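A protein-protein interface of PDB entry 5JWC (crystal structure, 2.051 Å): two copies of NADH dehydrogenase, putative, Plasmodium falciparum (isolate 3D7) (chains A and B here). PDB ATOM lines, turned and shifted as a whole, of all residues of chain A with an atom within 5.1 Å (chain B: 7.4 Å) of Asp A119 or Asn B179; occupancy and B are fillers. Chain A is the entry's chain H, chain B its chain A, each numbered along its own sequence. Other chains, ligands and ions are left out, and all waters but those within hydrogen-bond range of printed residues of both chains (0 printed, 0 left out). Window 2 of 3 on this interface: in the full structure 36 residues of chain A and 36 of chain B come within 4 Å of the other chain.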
ATOM      1  N   GLN A 102      13.466  15.860   6.017  1.00  0.00           N
ATOM      2  CA  GLN A 102      12.362  16.401   6.789  1.00  0.00           C
ATOM      3  C   GLN A 102      12.862  16.982   8.105  1.00  0.00           C
ATOM      4  O   GLN A 102      12.879  16.323   9.141  1.00  0.00           O
ATOM      5  CB  GLN A 102      11.288  15.351   7.037  1.00  0.00           C
ATOM      6  CG  GLN A 102      10.040  15.970   7.645  1.00  0.00           C
ATOM      7  CD  GLN A 102       8.837  15.042   7.607  1.00  0.00           C
ATOM      8  OE1 GLN A 102       7.754  15.428   7.152  1.00  0.00           O
ATOM      9  NE2 GLN A 102       9.015  13.825   8.086  1.00  0.00           N
ATOM     10  N   LEU A 103      13.261  18.240   8.048  1.00  0.00           N
ATOM     11  CA  LEU A 103      13.819  18.924   9.201  1.00  0.00           C
ATOM     12  C   LEU A 103      13.299  20.350   9.219  1.00  0.00           C
ATOM     13  O   LEU A 103      12.962  20.890   8.163  1.00  0.00           O
ATOM     14  CB  LEU A 103      15.348  18.923   9.146  1.00  0.00           C
ATOM     15  CG  LEU A 103      16.108  17.591   9.168  1.00  0.00           C
ATOM     16  CD1 LEU A 103      17.568  17.817   8.813  1.00  0.00           C
ATOM     17  CD2 LEU A 103      15.984  16.932  10.537  1.00  0.00           C
ATOM     18  N   CYS A 117      19.441  22.370  12.418  1.00  0.00           N
ATOM     19  CA  CYS A 117      18.056  21.946  12.263  1.00  0.00           C
ATOM     20  C   CYS A 117      17.645  21.047  13.411  1.00  0.00           C
ATOM     21  O   CYS A 117      18.491  20.538  14.142  1.00  0.00           O
ATOM     22  CB  CYS A 117      17.853  21.201  10.945  1.00  0.00           C
ATOM     23  SG  CYS A 117      18.321  22.117   9.481  1.00  0.00           S
ATOM     24  N   ILE A 118      16.343  20.840  13.561  1.00  0.00           N
ATOM     25  CA  ILE A 118      15.838  19.785  14.427  1.00  0.00           C
ATOM     26  C   ILE A 118      14.878  18.883  13.658  1.00  0.00           C
ATOM     27  O   ILE A 118      14.206  19.334  12.726  1.00  0.00           O
ATOM     28  CB  ILE A 118      15.097  20.333  15.660  1.00  0.00           C
ATOM     29  CG1 ILE A 118      14.033  21.341  15.213  1.00  0.00           C
ATOM     30  CG2 ILE A 118      16.074  20.951  16.635  1.00  0.00           C
ATOM     31  CD1 ILE A 118      13.079  21.773  16.296  1.00  0.00           C
ATOM     32  N   ASP A 119      14.811  17.612  14.055  1.00  0.00           N
ATOM     33  CA  ASP A 119      13.814  16.706  13.507  1.00  0.00           C
ATOM     34  C   ASP A 119      12.569  16.736  14.375  1.00  0.00           C
ATOM     35  O   ASP A 119      12.488  17.491  15.332  1.00  0.00           O
ATOM     36  CB  ASP A 119      14.357  15.274  13.358  1.00  0.00           C
ATOM     37  CG  ASP A 119      14.804  14.641  14.681  1.00  0.00           C
ATOM     38  OD1 ASP A 119      15.559  13.645  14.604  1.00  0.00           O
ATOM     39  OD2 ASP A 119      14.414  15.110  15.778  1.00  0.00           O
ATOM     40  N   ILE A 120      11.600  15.904  14.036  1.00  0.00           N
ATOM     41  CA  ILE A 120      10.308  15.925  14.701  1.00  0.00           C
ATOM     42  C   ILE A 120      10.428  15.527  16.185  1.00  0.00           C
ATOM     43  O   ILE A 120       9.538  15.804  16.981  1.00  0.00           O
ATOM     44  CB  ILE A 120       9.312  15.005  13.944  1.00  0.00           C
ATOM     45  CG1 ILE A 120       7.863  15.316  14.320  1.00  0.00           C
ATOM     46  CG2 ILE A 120       9.673  13.528  14.124  1.00  0.00           C
ATOM     47  CD1 ILE A 120       7.388  16.700  13.905  1.00  0.00           C
ATOM     48  N   GLU A 121      11.557  14.933  16.561  1.00  0.00           N
ATOM     49  CA  GLU A 121      11.801  14.522  17.943  1.00  0.00           C
ATOM     50  C   GLU A 121      12.772  15.458  18.678  1.00  0.00           C
ATOM     51  O   GLU A 121      13.305  15.115  19.738  1.00  0.00           O
ATOM     52  CB  GLU A 121      12.329  13.082  17.966  1.00  0.00           C
ATOM     53  CG  GLU A 121      11.339  12.055  17.408  1.00  0.00           C
ATOM     54  CD  GLU A 121      11.922  10.651  17.303  1.00  0.00           C
ATOM     55  OE1 GLU A 121      13.028  10.403  17.850  1.00  0.00           O
ATOM     56  OE2 GLU A 121      11.263   9.791  16.676  1.00  0.00           O
ATOM     57  N   ASN A 122      12.981  16.639  18.103  1.00  0.00           N
ATOM     58  CA  ASN A 122      13.843  17.674  18.664  1.00  0.00           C
ATOM     59  C   ASN A 122      15.311  17.291  18.691  1.00  0.00           C
ATOM     60  O   ASN A 122      16.106  17.944  19.356  1.00  0.00           O
ATOM     61  CB  ASN A 122      13.398  18.047  20.081  1.00  0.00           C
ATOM     62  CG  ASN A 122      12.019  18.668  20.109  1.00  0.00           C
ATOM     63  OD1 ASN A 122      11.751  19.643  19.402  1.00  0.00           O
ATOM     64  ND2 ASN A 122      11.128  18.100  20.916  1.00  0.00           N
ATOM     65  N   ASN A 123      15.680  16.253  17.953  1.00  0.00           N
ATOM     66  CA  ASN A 123      17.092  15.946  17.773  1.00  0.00           C
ATOM     67  C   ASN A 123      17.753  16.970  16.856  1.00  0.00           C
ATOM     68  O   ASN A 123      17.216  17.304  15.793  1.00  0.00           O
ATOM     69  CB  ASN A 123      17.272  14.542  17.205  1.00  0.00           C
ATOM     70  CG  ASN A 123      16.675  13.479  18.101  1.00  0.00           C
ATOM     71  OD1 ASN A 123      16.909  13.474  19.310  1.00  0.00           O
ATOM     72  ND2 ASN A 123      15.875  12.590  17.520  1.00  0.00           N
ATOM     73  N   LYS A 124      18.913  17.465  17.270  1.00  0.00           N
ATOM     74  CA  LYS A 124      19.609  18.496  16.521  1.00  0.00           C
ATOM     75  C   LYS A 124      20.437  17.918  15.384  1.00  0.00           C
ATOM     76  O   LYS A 124      21.090  16.882  15.525  1.00  0.00           O
ATOM     77  CB  LYS A 124      20.480  19.324  17.477  1.00  0.00           C
ATOM     78  CG  LYS A 124      21.192  20.509  16.846  1.00  0.00           C
ATOM     79  CD  LYS A 124      21.807  21.387  17.935  1.00  0.00           C
ATOM     80  CE  LYS A 124      22.965  22.227  17.422  1.00  0.00           C
ATOM     81  NZ  LYS A 124      23.412  23.225  18.445  1.00  0.00           N
ATOM     82  N   VAL A 125      20.395  18.599  14.244  1.00  0.00           N
ATOM     83  CA  VAL A 125      21.140  18.215  13.056  1.00  0.00           C
ATOM     84  C   VAL A 125      21.907  19.417  12.524  1.00  0.00           C
ATOM     85  O   VAL A 125      21.350  20.520  12.402  1.00  0.00           O
ATOM     86  CB  VAL A 125      20.204  17.673  11.947  1.00  0.00           C
ATOM     87  CG1 VAL A 125      21.008  17.144  10.776  1.00  0.00           C
ATOM     88  CG2 VAL A 125      19.292  16.579  12.511  1.00  0.00           C
ATOM     89  N   LYS B 174      11.758   9.391   8.799  1.00  0.00           N
ATOM     90  CA  LYS B 174      12.661   9.388   9.941  1.00  0.00           C
ATOM     91  C   LYS B 174      13.971   8.669   9.622  1.00  0.00           C
ATOM     92  O   LYS B 174      15.049   9.130  10.010  1.00  0.00           O
ATOM     93  CB  LYS B 174      11.977   8.744  11.143  1.00  0.00           C
ATOM     94  CG  LYS B 174      12.848   8.653  12.373  1.00  0.00           C
ATOM     95  CD  LYS B 174      12.109   7.974  13.514  1.00  0.00           C
ATOM     96  CE  LYS B 174      12.980   7.898  14.772  1.00  0.00           C
ATOM     97  NZ  LYS B 174      12.241   7.358  15.954  1.00  0.00           N
ATOM     98  N   CYS B 175      13.888   7.567   8.880  1.00  0.00           N
ATOM     99  CA  CYS B 175      15.070   6.771   8.538  1.00  0.00           C
ATOM    100  C   CYS B 175      15.896   7.322   7.380  1.00  0.00           C
ATOM    101  O   CYS B 175      16.922   6.749   7.030  1.00  0.00           O
ATOM    102  CB  CYS B 175      14.660   5.332   8.194  1.00  0.00           C
ATOM    103  SG  CYS B 175      14.074   4.441   9.630  1.00  0.00           S
ATOM    104  N   THR B 176      15.450   8.422   6.785  1.00  0.00           N
ATOM    105  CA  THR B 176      16.218   9.076   5.737  1.00  0.00           C
ATOM    106  C   THR B 176      17.140  10.148   6.368  1.00  0.00           C
ATOM    107  O   THR B 176      18.034  10.665   5.716  1.00  0.00           O
ATOM    108  CB  THR B 176      15.264   9.678   4.666  1.00  0.00           C
ATOM    109  OG1 THR B 176      14.533   8.603   4.057  1.00  0.00           O
ATOM    110  CG2 THR B 176      16.022  10.400   3.560  1.00  0.00           C
ATOM    111  N   LEU B 177      16.931  10.448   7.646  1.00  0.00           N
ATOM    112  CA  LEU B 177      17.759  11.431   8.354  1.00  0.00           C
ATOM    113  C   LEU B 177      19.184  10.923   8.617  1.00  0.00           C
ATOM    114  O   LEU B 177      19.402   9.719   8.738  1.00  0.00           O
ATOM    115  CB  LEU B 177      17.099  11.825   9.661  1.00  0.00           C
ATOM    116  CG  LEU B 177      15.697  12.406   9.474  1.00  0.00           C
ATOM    117  CD1 LEU B 177      15.110  12.827  10.824  1.00  0.00           C
ATOM    118  CD2 LEU B 177      15.723  13.575   8.477  1.00  0.00           C
ATOM    119  N   PRO B 178      20.161  11.844   8.705  1.00  0.00           N
ATOM    120  CA  PRO B 178      21.563  11.400   8.818  1.00  0.00           C
ATOM    121  C   PRO B 178      21.945  10.913  10.222  1.00  0.00           C
ATOM    122  O   PRO B 178      22.982  10.266  10.404  1.00  0.00           O
ATOM    123  CB  PRO B 178      22.352  12.661   8.443  1.00  0.00           C
ATOM    124  CG  PRO B 178      21.463  13.798   8.863  1.00  0.00           C
ATOM    125  CD  PRO B 178      20.048  13.315   8.606  1.00  0.00           C
ATOM    126  N   ASN B 179      21.097  11.218  11.194  1.00  0.00           N
ATOM    127  CA  ASN B 179      21.361  10.949  12.600  1.00  0.00           C
ATOM    128  C   ASN B 179      20.966   9.553  13.116  1.00  0.00           C
ATOM    129  O   ASN B 179      20.665   9.400  14.299  1.00  0.00           O
ATOM    130  CB  ASN B 179      20.648  12.016  13.454  1.00  0.00           C
ATOM    131  CG  ASN B 179      19.116  12.051  13.224  1.00  0.00           C
ATOM    132  OD1 ASN B 179      18.512  11.077  12.769  1.00  0.00           O
ATOM    133  ND2 ASN B 179      18.493  13.175  13.567  1.00  0.00           N
ATOM    134  N   ILE B 180      21.003   8.549  12.236  1.00  0.00           N
ATOM    135  CA  ILE B 180      20.519   7.202  12.559  1.00  0.00           C
ATOM    136  C   ILE B 180      21.370   6.118  11.885  1.00  0.00           C
ATOM    137  O   ILE B 180      21.652   6.197  10.692  1.00  0.00           O
ATOM    138  CB  ILE B 180      19.024   7.051  12.154  1.00  0.00           C
ATOM    139  CG1 ILE B 180      18.127   7.752  13.181  1.00  0.00           C
ATOM    140  CG2 ILE B 180      18.622   5.587  12.047  1.00  0.00           C
ATOM    141  CD1 ILE B 180      16.784   8.221  12.636  1.00  0.00           C
ATOM    142  N   SER B 181      21.789   5.114  12.656  1.00  0.00           N
ATOM    143  CA  SER B 181      22.632   4.040  12.129  1.00  0.00           C
ATOM    144  C   SER B 181      21.841   3.021  11.332  1.00  0.00           C
ATOM    145  O   SER B 181      20.616   2.954  11.427  1.00  0.00           O
ATOM    146  CB  SER B 181      23.348   3.312  13.263  1.00  0.00           C
ATOM    147  OG  SER B 181      22.402   2.664  14.099  1.00  0.00           O
ATOM    148  N   GLU B 184      19.852   0.694  13.555  1.00  0.00           N
ATOM    149  CA  GLU B 184      18.618   1.281  14.063  1.00  0.00           C
ATOM    150  C   GLU B 184      17.554   1.299  12.972  1.00  0.00           C
ATOM    151  O   GLU B 184      16.370   1.146  13.259  1.00  0.00           O
ATOM    152  CB  GLU B 184      18.834   2.708  14.580  1.00  0.00           C
ATOM    153  CG  GLU B 184      19.773   2.836  15.768  1.00  0.00           C
ATOM    154  CD  GLU B 184      20.291   4.269  15.947  1.00  0.00           C
ATOM    155  OE1 GLU B 184      21.029   4.776  15.065  1.00  0.00           O
ATOM    156  OE2 GLU B 184      19.927   4.902  16.963  1.00  0.00           O
ATOM    157  N   LYS B 185      17.995   1.482  11.730  1.00  0.00           N
ATOM    158  CA  LYS B 185      17.105   1.491  10.576  1.00  0.00           C
ATOM    159  C   LYS B 185      16.454   0.123  10.371  1.00  0.00           C
ATOM    160  O   LYS B 185      15.241   0.035  10.148  1.00  0.00           O
ATOM    161  CB  LYS B 185      17.858   1.899   9.304  1.00  0.00           C
ATOM    162  CG  LYS B 185      18.291   3.363   9.226  1.00  0.00           C
ATOM    163  CD  LYS B 185      18.872   3.675   7.846  1.00  0.00           C
ATOM    164  CE  LYS B 185      19.815   4.874   7.881  1.00  0.00           C
ATOM    165  NZ  LYS B 185      20.320   5.269   6.533  1.00  0.00           N
ATOM    166  N   MET B 188      13.794  -0.226  12.899  1.00  0.00           N
ATOM    167  CA  MET B 188      12.659   0.671  12.691  1.00  0.00           C
ATOM    168  C   MET B 188      11.868   0.327  11.434  1.00  0.00           C
ATOM    169  O   MET B 188      10.671   0.563  11.378  1.00  0.00           O
ATOM    170  CB  MET B 188      13.127   2.121  12.611  1.00  0.00           C
ATOM    171  CG  MET B 188      13.181   2.823  13.951  1.00  0.00           C
ATOM    172  SD  MET B 188      13.740   4.535  13.759  1.00  0.00           S
ATOM    173  CE  MET B 188      15.486   4.281  13.465  1.00  0.00           C
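OE2 of Glu A121 lies within salt-bridge range of NZ of Lys B174, at 2.7 Å.
ND2 of Asn B179 lies within hydrogen-bond range of OD1 of Asp A119 (3.1 Å).
The backbone carbonyl oxygen of Val A125 lies within hydrogen-bond range of the backbone NH of Cys A117 (2.7 Å).
The side-chain carboxylate of Asp A119 is in hydrogen-bond range of the backbone NH of Glu A121 (3.0 Å).
N of Asn A122 lies within hydrogen-bond range of OD2 of Asp A119 (3.1 Å).
The side-chain carboxylate (OD2) of Asp A119 sits at hydrogen-bond distance from the backbone NH (N) of Asn A123 (2.8 Å).
Leu A103 touches Leu B177 (CD2 to CD2, 3.9 Å).
Asp A119 touches Leu B177 (CB to CD1, 3.6 Å).
Pro B178 touches Val A125.
Asn B179 touches Val A125.
Ile A120 touches none of the printed residues of chain B.
Of the printed residues of chain B, Val A125 touches Pro B178 and Asn B179.
Of the printed residues of chain A, Leu B177 touches Leu A103 (3.9 Å) and Asp A119 (3.6 Å).
Asn B179 touches just these residues of chain A: Asp A119 (3.1 Å) and Val A125 (3.7 Å).
The nearest residue of chain A that does not touch Asn B179 is Asn A123 (4.1 Å).
The nearest printed residue of chain B that does not touch Glu A121 is Met B188 (6.5 Å).
Hydrophobic or aromatic side chains of chain B that line the printed part of chain A: Leu B177 and Pro B178.
Printed residues of chain A that touch a printed residue of chain B: Leu A103, Asp A119, Glu A121 and Val A125.
No position is printed for both chains.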
